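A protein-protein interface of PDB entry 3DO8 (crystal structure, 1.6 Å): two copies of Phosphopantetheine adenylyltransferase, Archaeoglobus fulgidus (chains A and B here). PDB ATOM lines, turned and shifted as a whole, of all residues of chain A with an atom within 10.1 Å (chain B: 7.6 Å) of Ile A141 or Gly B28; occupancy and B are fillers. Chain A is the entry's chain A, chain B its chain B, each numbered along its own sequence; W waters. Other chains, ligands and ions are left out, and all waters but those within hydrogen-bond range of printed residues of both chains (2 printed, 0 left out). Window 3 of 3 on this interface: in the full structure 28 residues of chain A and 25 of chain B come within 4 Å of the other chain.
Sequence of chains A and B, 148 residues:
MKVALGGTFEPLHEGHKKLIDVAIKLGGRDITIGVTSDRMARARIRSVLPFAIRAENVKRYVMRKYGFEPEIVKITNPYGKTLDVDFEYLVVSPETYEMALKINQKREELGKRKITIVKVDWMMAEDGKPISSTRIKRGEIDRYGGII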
ATOM      1  N   ASP A  21     -24.848  -5.621  11.440  1.00  0.00           N
ATOM      2  CA  ASP A  21     -24.362  -6.924  10.945  1.00  0.00           C
ATOM      3  C   ASP A  21     -24.686  -7.048   9.458  1.00  0.00           C
ATOM      4  O   ASP A  21     -23.871  -7.471   8.661  1.00  0.00           O
ATOM      5  CB  ASP A  21     -25.025  -8.081  11.690  1.00  0.00           C
ATOM      6  CG  ASP A  21     -24.362  -9.417  11.398  1.00  0.00           C
ATOM      7  OD1 ASP A  21     -23.144  -9.535  11.676  1.00  0.00           O
ATOM      8  OD2 ASP A  21     -25.072 -10.349  10.894  1.00  0.00           O
ATOM      9  N   VAL A  22     -25.918  -6.734   9.102  1.00  0.00           N
ATOM     10  CA  VAL A  22     -26.344  -6.851   7.698  1.00  0.00           C
ATOM     11  C   VAL A  22     -25.487  -5.891   6.843  1.00  0.00           C
ATOM     12  O   VAL A  22     -24.970  -6.271   5.809  1.00  0.00           O
ATOM     13  CB  VAL A  22     -27.881  -6.592   7.524  1.00  0.00           C
ATOM     14  CG1 VAL A  22     -28.246  -6.396   6.057  1.00  0.00           C
ATOM     15  CG2 VAL A  22     -28.695  -7.701   8.194  1.00  0.00           C
ATOM     16  N   ILE A  24     -22.478  -4.659   7.325  1.00  0.00           N
ATOM     17  CA  ILE A  24     -21.098  -5.094   7.209  1.00  0.00           C
ATOM     18  C   ILE A  24     -20.947  -6.342   6.354  1.00  0.00           C
ATOM     19  O   ILE A  24     -19.980  -6.468   5.593  1.00  0.00           O
ATOM     20  CB  ILE A  24     -20.428  -5.253   8.596  1.00  0.00           C
ATOM     21  CG1 ILE A  24     -20.335  -3.867   9.254  1.00  0.00           C
ATOM     22  CG2 ILE A  24     -19.078  -5.897   8.452  1.00  0.00           C
ATOM     23  CD1 ILE A  24     -19.793  -3.820  10.695  1.00  0.00           C
ATOM     24  N   LYS A  25     -21.889  -7.265   6.467  1.00  0.00           N
ATOM     25  CA  LYS A  25     -21.883  -8.427   5.610  1.00  0.00           C
ATOM     26  C   LYS A  25     -22.047  -8.009   4.148  1.00  0.00           C
ATOM     27  O   LYS A  25     -21.394  -8.577   3.259  1.00  0.00           O
ATOM     28  CB  LYS A  25     -22.914  -9.464   6.083  1.00  0.00           C
ATOM     29  CG  LYS A  25     -22.430 -10.184   7.352  1.00  0.00           C
ATOM     30  CD  LYS A  25     -23.448 -11.066   8.020  1.00  0.00           C
ATOM     31  CE  LYS A  25     -22.776 -11.843   9.162  1.00  0.00           C
ATOM     32  NZ  LYS A  25     -23.750 -12.479  10.076  1.00  0.00           N
ATOM     33  N   LEU A  26     -22.858  -6.988   3.882  1.00  0.00           N
ATOM     34  CA  LEU A  26     -23.055  -6.527   2.513  1.00  0.00           C
ATOM     35  C   LEU A  26     -21.868  -5.756   1.982  1.00  0.00           C
ATOM     36  O   LEU A  26     -21.541  -5.894   0.798  1.00  0.00           O
ATOM     37  CB  LEU A  26     -24.306  -5.633   2.385  1.00  0.00           C
ATOM     38  CG  LEU A  26     -25.646  -6.339   2.528  1.00  0.00           C
ATOM     39  CD1 LEU A  26     -26.803  -5.303   2.530  1.00  0.00           C
ATOM     40  CD2 LEU A  26     -25.849  -7.404   1.445  1.00  0.00           C
ATOM     41  N   GLY A  27     -21.275  -4.896   2.819  1.00  0.00           N
ATOM     42  CA  GLY A  27     -20.318  -3.883   2.361  1.00  0.00           C
ATOM     43  C   GLY A  27     -18.888  -4.015   2.831  1.00  0.00           C
ATOM     44  O   GLY A  27     -17.997  -3.355   2.291  1.00  0.00           O
ATOM     45  N   GLY A  28     -18.662  -4.833   3.855  1.00  0.00           N
ATOM     46  CA  GLY A  28     -17.342  -4.935   4.468  1.00  0.00           C
ATOM     47  C   GLY A  28     -16.941  -3.592   5.033  1.00  0.00           C
ATOM     48  O   GLY A  28     -17.715  -2.944   5.691  1.00  0.00           O
ATOM     49  N   LYS A  65     -16.508  -6.272  17.634  1.00  0.00           N
ATOM     50  CA  LYS A  65     -17.180  -7.404  16.956  1.00  0.00           C
ATOM     51  C   LYS A  65     -16.675  -7.706  15.557  1.00  0.00           C
ATOM     52  O   LYS A  65     -16.746  -8.844  15.113  1.00  0.00           O
ATOM     53  CB  LYS A  65     -18.696  -7.195  16.912  1.00  0.00           C
ATOM     54  CG  LYS A  65     -19.346  -7.213  18.260  1.00  0.00           C
ATOM     55  CD  LYS A  65     -19.248  -8.567  18.933  1.00  0.00           C
ATOM     56  CE  LYS A  65     -20.092  -8.633  20.202  1.00  0.00           C
ATOM     57  NZ  LYS A  65     -19.989 -10.004  20.814  1.00  0.00           N
ATOM     58  N   TYR A  66     -16.170  -6.696  14.862  1.00  0.00           N
ATOM     59  CA  TYR A  66     -15.786  -6.831  13.452  1.00  0.00           C
ATOM     60  C   TYR A  66     -14.349  -6.494  13.124  1.00  0.00           C
ATOM     61  O   TYR A  66     -13.911  -6.747  11.995  1.00  0.00           O
ATOM     62  CB  TYR A  66     -16.697  -6.006  12.533  1.00  0.00           C
ATOM     63  CG  TYR A  66     -18.140  -6.435  12.665  1.00  0.00           C
ATOM     64  CD1 TYR A  66     -18.652  -7.484  11.897  1.00  0.00           C
ATOM     65  CD2 TYR A  66     -19.010  -5.831  13.586  1.00  0.00           C
ATOM     66  CE1 TYR A  66     -19.993  -7.900  12.030  1.00  0.00           C
ATOM     67  CE2 TYR A  66     -20.323  -6.258  13.715  1.00  0.00           C
ATOM     68  CZ  TYR A  66     -20.803  -7.313  12.971  1.00  0.00           C
ATOM     69  OH  TYR A  66     -22.149  -7.686  13.120  1.00  0.00           O
ATOM     70  N   ILE A 136     -27.889 -14.695  15.854  1.00  0.00           N
ATOM     71  CA  ILE A 136     -27.113 -14.391  14.663  1.00  0.00           C
ATOM     72  C   ILE A 136     -25.639 -14.334  15.056  1.00  0.00           C
ATOM     73  O   ILE A 136     -25.258 -13.597  15.977  1.00  0.00           O
ATOM     74  CB  ILE A 136     -27.486 -13.040  14.041  1.00  0.00           C
ATOM     75  CG1 ILE A 136     -28.937 -13.039  13.537  1.00  0.00           C
ATOM     76  CG2 ILE A 136     -26.534 -12.726  12.899  1.00  0.00           C
ATOM     77  CD1 ILE A 136     -29.570 -11.655  13.518  1.00  0.00           C
ATOM     78  N   LYS A 137     -24.817 -15.111  14.361  1.00  0.00           N
ATOM     79  CA  LYS A 137     -23.382 -15.068  14.571  1.00  0.00           C
ATOM     80  C   LYS A 137     -22.808 -13.815  13.894  1.00  0.00           C
ATOM     81  O   LYS A 137     -22.734 -13.742  12.659  1.00  0.00           O
ATOM     82  CB  LYS A 137     -22.741 -16.344  14.031  1.00  0.00           C
ATOM     83  CG  LYS A 137     -23.236 -17.603  14.757  1.00  0.00           C
ATOM     84  CD  LYS A 137     -22.399 -17.943  15.985  1.00  0.00           C
ATOM     85  CE  LYS A 137     -21.078 -18.597  15.594  1.00  0.00           C
ATOM     86  NZ  LYS A 137     -20.474 -19.380  16.716  1.00  0.00           N
ATOM     87  N   ARG A 138     -22.435 -12.827  14.713  1.00  0.00           N
ATOM     88  CA  ARG A 138     -21.846 -11.574  14.215  1.00  0.00           C
ATOM     89  C   ARG A 138     -20.457 -11.795  13.669  1.00  0.00           C
ATOM     90  O   ARG A 138     -19.673 -12.559  14.225  1.00  0.00           O
ATOM     91  CB  ARG A 138     -21.724 -10.520  15.320  1.00  0.00           C
ATOM     92  CG  ARG A 138     -23.000 -10.197  16.040  1.00  0.00           C
ATOM     93  CD  ARG A 138     -24.158 -10.113  15.096  1.00  0.00           C
ATOM     94  NE  ARG A 138     -25.304  -9.464  15.728  1.00  0.00           N
ATOM     95  CZ  ARG A 138     -26.494  -9.299  15.155  1.00  0.00           C
ATOM     96  NH1 ARG A 138     -26.742  -9.749  13.923  1.00  0.00           N
ATOM     97  NH2 ARG A 138     -27.445  -8.689  15.829  1.00  0.00           N
ATOM     98  N   GLY A 139     -20.158 -11.097  12.585  1.00  0.00           N
ATOM     99  CA  GLY A 139     -18.842 -11.137  11.970  1.00  0.00           C
ATOM    100  C   GLY A 139     -18.991 -11.010  10.471  1.00  0.00           C
ATOM    101  O   GLY A 139     -20.098 -10.889   9.955  1.00  0.00           O
ATOM    102  N   GLU A 140     -17.868 -10.989   9.772  1.00  0.00           N
ATOM    103  CA  GLU A 140     -17.877 -11.142   8.333  1.00  0.00           C
ATOM    104  C   GLU A 140     -17.815 -12.651   8.103  1.00  0.00           C
ATOM    105  O   GLU A 140     -17.329 -13.383   8.969  1.00  0.00           O
ATOM    106  CB  GLU A 140     -16.702 -10.374   7.728  1.00  0.00           C
ATOM    107  CG  GLU A 140     -16.825  -8.881   8.031  1.00  0.00           C
ATOM    108  CD  GLU A 140     -15.638  -8.039   7.591  1.00  0.00           C
ATOM    109  OE1 GLU A 140     -14.699  -7.868   8.412  1.00  0.00           O
ATOM    110  OE2 GLU A 140     -15.681  -7.507   6.450  1.00  0.00           O
ATOM    111  N   ILE A 141     -18.353 -13.119   6.980  1.00  0.00           N
ATOM    112  CA  ILE A 141     -18.448 -14.560   6.719  1.00  0.00           C
ATOM    113  C   ILE A 141     -17.220 -15.123   5.956  1.00  0.00           C
ATOM    114  O   ILE A 141     -16.844 -16.280   6.161  1.00  0.00           O
ATOM    115  CB  ILE A 141     -19.777 -14.922   5.957  1.00  0.00           C
ATOM    116  CG1 ILE A 141     -19.742 -14.426   4.514  1.00  0.00           C
ATOM    117  CG2 ILE A 141     -21.019 -14.355   6.678  1.00  0.00           C
ATOM    118  CD1 ILE A 141     -20.966 -14.787   3.746  1.00  0.00           C
ATOM    119  N   ASP A 142     -16.617 -14.294   5.098  1.00  0.00           N
ATOM    120  CA  ASP A 142     -15.586 -14.695   4.088  1.00  0.00           C
ATOM    121  C   ASP A 142     -15.032 -16.131   4.139  1.00  0.00           C
ATOM    122  O   ASP A 142     -14.134 -16.500   3.340  1.00  0.00           O
ATOM    123  CB  ASP A 142     -14.414 -13.687   4.080  1.00  0.00           C
ATOM    124  CG  ASP A 142     -13.781 -13.509   5.438  1.00  0.00           C
ATOM    125  OD1 ASP A 142     -14.446 -13.875   6.416  1.00  0.00           O
ATOM    126  OD2 ASP A 142     -12.633 -13.009   5.546  1.00  0.00           O
ATOM    127  N   LYS B   2     -27.554 -20.560   7.959  1.00  0.00           N
ATOM    128  CA  LYS B   2     -27.474 -19.132   8.243  1.00  0.00           C
ATOM    129  C   LYS B   2     -28.686 -18.456   7.654  1.00  0.00           C
ATOM    130  O   LYS B   2     -29.381 -17.725   8.356  1.00  0.00           O
ATOM    131  CB  LYS B   2     -26.190 -18.506   7.629  1.00  0.00           C
ATOM    132  CG  LYS B   2     -25.012 -18.621   8.517  1.00  0.00           C
ATOM    133  CD  LYS B   2     -23.717 -18.162   7.877  1.00  0.00           C
ATOM    134  CE  LYS B   2     -22.734 -17.723   8.976  1.00  0.00           C
ATOM    135  NZ  LYS B   2     -22.975 -18.431  10.286  1.00  0.00           N
ATOM    136  N   VAL B   3     -28.915 -18.669   6.354  1.00  0.00           N
ATOM    137  CA  VAL B   3     -29.890 -17.868   5.606  1.00  0.00           C
ATOM    138  C   VAL B   3     -30.900 -18.751   4.877  1.00  0.00           C
ATOM    139  O   VAL B   3     -30.523 -19.763   4.286  1.00  0.00           O
ATOM    140  CB  VAL B   3     -29.195 -16.974   4.554  1.00  0.00           C
ATOM    141  CG1 VAL B   3     -30.267 -16.261   3.695  1.00  0.00           C
ATOM    142  CG2 VAL B   3     -28.224 -15.994   5.219  1.00  0.00           C
ATOM    143  N   ASP B  21     -27.828 -11.868  -4.300  1.00  0.00           N
ATOM    144  CA  ASP B  21     -26.603 -11.192  -3.828  1.00  0.00           C
ATOM    145  C   ASP B  21     -26.645 -10.956  -2.312  1.00  0.00           C
ATOM    146  O   ASP B  21     -25.682 -11.252  -1.613  1.00  0.00           O
ATOM    147  CB  ASP B  21     -26.389  -9.860  -4.514  1.00  0.00           C
ATOM    148  CG  ASP B  21     -25.004  -9.291  -4.267  1.00  0.00           C
ATOM    149  OD1 ASP B  21     -24.021  -9.991  -4.621  1.00  0.00           O
ATOM    150  OD2 ASP B  21     -24.905  -8.153  -3.723  1.00  0.00           O
ATOM    151  N   VAL B  22     -27.748 -10.403  -1.813  1.00  0.00           N
ATOM    152  CA  VAL B  22     -27.896 -10.167  -0.384  1.00  0.00           C
ATOM    153  C   VAL B  22     -27.822 -11.516   0.399  1.00  0.00           C
ATOM    154  O   VAL B  22     -27.099 -11.622   1.405  1.00  0.00           O
ATOM    155  CB  VAL B  22     -29.208  -9.394  -0.089  1.00  0.00           C
ATOM    156  CG1 VAL B  22     -29.486  -9.401   1.411  1.00  0.00           C
ATOM    157  CG2 VAL B  22     -29.121  -8.011  -0.704  1.00  0.00           C
ATOM    158  N   ALA B  23     -28.522 -12.547  -0.083  1.00  0.00           N
ATOM    159  CA  ALA B  23     -28.502 -13.877   0.588  1.00  0.00           C
ATOM    160  C   ALA B  23     -27.086 -14.445   0.657  1.00  0.00           C
ATOM    161  O   ALA B  23     -26.660 -14.969   1.693  1.00  0.00           O
ATOM    162  CB  ALA B  23     -29.441 -14.847  -0.108  1.00  0.00           C
ATOM    163  N   ILE B  24     -26.336 -14.327  -0.440  1.00  0.00           N
ATOM    164  CA  ILE B  24     -24.966 -14.874  -0.444  1.00  0.00           C
ATOM    165  C   ILE B  24     -24.017 -14.072   0.429  1.00  0.00           C
ATOM    166  O   ILE B  24     -23.153 -14.634   1.138  1.00  0.00           O
ATOM    167  CB  ILE B  24     -24.411 -15.044  -1.885  1.00  0.00           C
ATOM    168  CG1 ILE B  24     -25.234 -16.103  -2.608  1.00  0.00           C
ATOM    169  CG2 ILE B  24     -22.964 -15.431  -1.831  1.00  0.00           C
ATOM    170  CD1 ILE B  24     -24.937 -16.247  -4.076  1.00  0.00           C
ATOM    171  N   LYS B  25     -24.184 -12.760   0.424  1.00  0.00           N
ATOM    172  CA  LYS B  25     -23.391 -11.915   1.334  1.00  0.00           C
ATOM    173  C   LYS B  25     -23.672 -12.228   2.799  1.00  0.00           C
ATOM    174  O   LYS B  25     -22.761 -12.207   3.639  1.00  0.00           O
ATOM    175  CB  LYS B  25     -23.546 -10.450   1.002  1.00  0.00           C
ATOM    176  CG  LYS B  25     -22.834 -10.140  -0.306  1.00  0.00           C
ATOM    177  CD  LYS B  25     -23.170  -8.826  -0.922  1.00  0.00           C
ATOM    178  CE  LYS B  25     -22.136  -8.482  -1.989  1.00  0.00           C
ATOM    179  NZ  LYS B  25     -22.524  -7.211  -2.642  1.00  0.00           N
ATOM    180  N   LEU B  26     -24.918 -12.534   3.114  1.00  0.00           N
ATOM    181  CA  LEU B  26     -25.286 -12.865   4.487  1.00  0.00           C
ATOM    182  C   LEU B  26     -24.956 -14.297   4.861  1.00  0.00           C
ATOM    183  O   LEU B  26     -24.646 -14.557   6.036  1.00  0.00           O
ATOM    184  CB  LEU B  26     -26.783 -12.594   4.734  1.00  0.00           C
ATOM    185  CG  LEU B  26     -27.240 -11.147   4.689  1.00  0.00           C
ATOM    186  CD1 LEU B  26     -28.762 -11.032   4.947  1.00  0.00           C
ATOM    187  CD2 LEU B  26     -26.417 -10.241   5.582  1.00  0.00           C
ATOM    188  N   GLY B  27     -25.033 -15.233   3.908  1.00  0.00           N
ATOM    189  CA  GLY B  27     -24.949 -16.647   4.218  1.00  0.00           C
ATOM    190  C   GLY B  27     -23.730 -17.373   3.720  1.00  0.00           C
ATOM    191  O   GLY B  27     -23.437 -18.481   4.188  1.00  0.00           O
ATOM    192  N   GLY B  28     -23.021 -16.789   2.775  1.00  0.00           N
ATOM    193  CA  GLY B  28     -21.852 -17.433   2.216  1.00  0.00           C
ATOM    194  C   GLY B  28     -22.156 -18.584   1.281  1.00  0.00           C
ATOM    195  O   GLY B  28     -23.277 -18.763   0.836  1.00  0.00           O
ATOM    196  N   ARG B  29     -21.108 -19.342   0.998  1.00  0.00           N
ATOM    197  CA  ARG B  29     -21.041 -20.274  -0.120  1.00  0.00           C
ATOM    198  C   ARG B  29     -21.710 -21.506   0.301  1.00  0.00           C
ATOM    199  O   ARG B  29     -21.922 -22.407  -0.427  1.00  0.00           O
ATOM    200  CB  ARG B  29     -19.586 -20.455  -0.551  1.00  0.00           C
ATOM    201  CG  ARG B  29     -19.052 -19.093  -1.032  1.00  0.00           C
ATOM    202  CD  ARG B  29     -17.641 -18.951  -1.566  1.00  0.00           C
ATOM    203  NE  ARG B  29     -17.308 -19.700  -2.765  1.00  0.00           N
ATOM    204  CZ  ARG B  29     -16.972 -19.193  -3.961  1.00  0.00           C
ATOM    205  NH1 ARG B  29     -16.654 -19.993  -4.933  1.00  0.00           N
ATOM    206  NH2 ARG B  29     -16.939 -17.909  -4.194  1.00  0.00           N
ATOM    207  N   ASP B  30     -22.118 -21.400   1.525  1.00  0.00           N
ATOM    208  CA  ASP B  30     -22.988 -22.209   2.314  1.00  0.00           C
ATOM    209  C   ASP B  30     -24.354 -22.546   1.850  1.00  0.00           C
ATOM    210  O   ASP B  30     -24.876 -23.630   2.062  1.00  0.00           O
ATOM    211  CB  ASP B  30     -23.304 -21.297   3.507  1.00  0.00           C
ATOM    212  CG  ASP B  30     -23.318 -22.015   4.800  1.00  0.00           C
ATOM    213  OD1 ASP B  30     -22.256 -22.553   5.177  1.00  0.00           O
ATOM    214  OD2 ASP B  30     -24.387 -22.039   5.428  1.00  0.00           O
ATOM    215  N   ILE B  31     -25.007 -21.515   1.388  1.00  0.00           N
ATOM    216  CA  ILE B  31     -26.428 -21.423   1.430  1.00  0.00           C
ATOM    217  C   ILE B  31     -27.063 -22.522   0.616  1.00  0.00           C
ATOM    218  O   ILE B  31     -26.519 -22.995  -0.397  1.00  0.00           O
ATOM    219  CB  ILE B  31     -26.932 -20.057   0.876  1.00  0.00           C
ATOM    220  CG1 ILE B  31     -26.339 -19.834  -0.512  1.00  0.00           C
ATOM    221  CG2 ILE B  31     -26.507 -18.970   1.713  1.00  0.00           C
ATOM    222  CD1 ILE B  31     -27.167 -18.964  -1.400  1.00  0.00           C
ATOM    223  N   THR B  32     -28.235 -22.868   1.069  1.00  0.00           N
ATOM    224  CA  THR B  32     -29.189 -23.587   0.240  1.00  0.00           C
ATOM    225  C   THR B  32     -30.272 -22.601  -0.200  1.00  0.00           C
ATOM    226  O   THR B  32     -30.810 -21.853   0.605  1.00  0.00           O
ATOM    227  CB  THR B  32     -29.849 -24.798   0.965  1.00  0.00           C
ATOM    228  OG1 THR B  32     -30.862 -24.337   1.891  1.00  0.00           O
ATOM    229  CG2 THR B  32     -28.773 -25.652   1.684  1.00  0.00           C
ATOM    230  N   PHE B  68     -19.543 -20.672  -7.283  1.00  0.00           N
ATOM    231  CA  PHE B  68     -19.954 -21.925  -6.667  1.00  0.00           C
ATOM    232  C   PHE B  68     -21.338 -22.353  -7.107  1.00  0.00           C
ATOM    233  O   PHE B  68     -22.166 -21.523  -7.509  1.00  0.00           O
ATOM    234  CB  PHE B  68     -19.859 -21.856  -5.137  1.00  0.00           C
ATOM    235  CG  PHE B  68     -20.919 -21.002  -4.482  1.00  0.00           C
ATOM    236  CD1 PHE B  68     -22.028 -21.601  -3.931  1.00  0.00           C
ATOM    237  CD2 PHE B  68     -20.797 -19.636  -4.412  1.00  0.00           C
ATOM    238  CE1 PHE B  68     -23.038 -20.826  -3.337  1.00  0.00           C
ATOM    239  CE2 PHE B  68     -21.793 -18.859  -3.799  1.00  0.00           C
ATOM    240  CZ  PHE B  68     -22.885 -19.467  -3.265  1.00  0.00           C
ATOM    241  N   PRO B  70     -24.705 -23.481  -5.842  1.00  0.00           N
ATOM    242  CA  PRO B  70     -25.485 -23.510  -4.610  1.00  0.00           C
ATOM    243  C   PRO B  70     -26.289 -24.777  -4.476  1.00  0.00           C
ATOM    244  O   PRO B  70     -26.641 -25.396  -5.477  1.00  0.00           O
ATOM    245  CB  PRO B  70     -26.454 -22.336  -4.783  1.00  0.00           C
ATOM    246  CG  PRO B  70     -26.682 -22.311  -6.292  1.00  0.00           C
ATOM    247  CD  PRO B  70     -25.282 -22.546  -6.829  1.00  0.00           C
ATOM    248  N   GLU B  88     -30.678 -17.651  10.868  1.00  0.00           N
ATOM    249  CA  GLU B  88     -30.297 -16.315  11.327  1.00  0.00           C
ATOM    250  C   GLU B  88     -31.056 -15.230  10.574  1.00  0.00           C
ATOM    251  O   GLU B  88     -31.490 -14.264  11.162  1.00  0.00           O
ATOM    252  CB  GLU B  88     -28.800 -16.038  11.119  1.00  0.00           C
ATOM    253  CG  GLU B  88     -27.849 -17.073  11.736  1.00  0.00           C
ATOM    254  CD  GLU B  88     -26.368 -16.717  11.599  1.00  0.00           C
ATOM    255  OE1 GLU B  88     -25.969 -15.969  10.668  1.00  0.00           O
ATOM    256  OE2 GLU B  88     -25.590 -17.199  12.461  1.00  0.00           O
HETATM  257  O   HOH W   1     -20.422 -11.081   3.333  1.00  0.00           O
HETATM  258  O   HOH W   2     -25.432 -14.195   8.592  1.00  0.00           O
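Of the printed residues of chain B, Leu A26 touches Val B22 (3.9 Å) and Lys B25 (3.8 Å). Of the printed residues of chain B, Ile A136 touches Glu B88. Of the printed residues of chain B, Lys A137 touches Glu B88 (2.9 Å). Of chain B, only Ile B24 (3.4 Å), Lys B25 (3.1 Å), Leu B26 (3.7 Å), Gly B27 (3.8 Å) and Gly B28 (3.0 Å) come within 4 Å of Ile A141. Asp A142 touches none of the printed residues of chain B. Of chain A, only Ile A141 comes within 4 Å of Ile B24. Printed residues of chain A within 4 Å of Leu B26: Val A22, Lys A25 and Ile A141. Gly B27 touches just one residue of chain A: Ile A141 (3.8 Å). Gly B28 touches just one residue of chain A: Ile A141 (3.0 Å). No residue of chain A comes within 4 Å of Asp B30. Ile B31 touches none of the printed residues of chain A. The nearest printed residue of chain B that does not touch Ile A136 is Lys B2 (6.8 Å).
Hydrophobic or aromatic side chains of chain A within 4 Å of the printed part of chain B: Leu A26, Ile A136 and Ile A141. Of the 17 printed residues of chain B, 7 touch a printed residue of chain A. Hydrophobic or aromatic side chains of chain B that line the printed part of chain A: Val B22 and Leu B26.
Val A22 touches Leu B26, and with the chains exchanged Leu A26 touches Val B22. Lys B25 touches its own counterpart, Lys A25. Lys A25 touches Leu B26, and with the chains exchanged Leu A26 touches Lys B25. Positions printed for both chains: 21, 22, 24, 25, 26, 27 and 28. Of the 12 pairs that touch across the chains among the printed residues, 5 have their exchanged pair printed and touching as well.
The side-chain carboxylate (OD2) of Asp A21 lies within salt-bridge range of the side-chain amino group (NZ) of Lys A25, at 2.6 Å. The backbone carbonyl oxygen of Lys A137 sits at hydrogen-bond distance from the side-chain amino group of Lys A25, at 3.0 Å. The side-chain amino group of Lys B2 lies within salt-bridge range of the side-chain carboxylate of Glu B88 (3.6 Å). The side-chain amino group (NZ) of Lys B25 is in salt-bridge range of the side-chain carboxylate (OD2) of Asp B21.
OE2 of Glu B88 lies within hydrogen-bond range of N of Lys A137, 2.9 Å away.
Among the printed residues, pairs that only touch across the chains: Val A22 with Leu B26 (3.997 Å), Lys A25 with Lys B25 (3.6 Å), Lys A25 with Leu B26 (3.6 Å), Leu A26 with Val B22 (3.9 Å), Leu A26 with Lys B25 (3.8 Å), Ile A136 with Glu B88 (3.7 Å), Ile A141 with Ile B24 (3.4 Å), Ile A141 with Lys B25 (3.1 Å), Ile A141 with Leu B26 (3.7 Å), Ile A141 with Gly B27 (3.8 Å) and Ile A141 with Gly B28 (3.0 Å).
Water W1 lies within hydrogen-bond range of the backbone carbonyl oxygen of Lys B25 (2.6 Å) and the backbone carbonyl oxygen of Lys A25 (2.7 Å). Water W2 lies within hydrogen-bond range of the backbone carbonyl oxygen (O) of Leu B26 (2.7 Å), the side-chain carboxylate (OE1) of Glu B88 (2.8 Å) and the side-chain amino group (NZ) of Lys A25 (2.8 Å).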
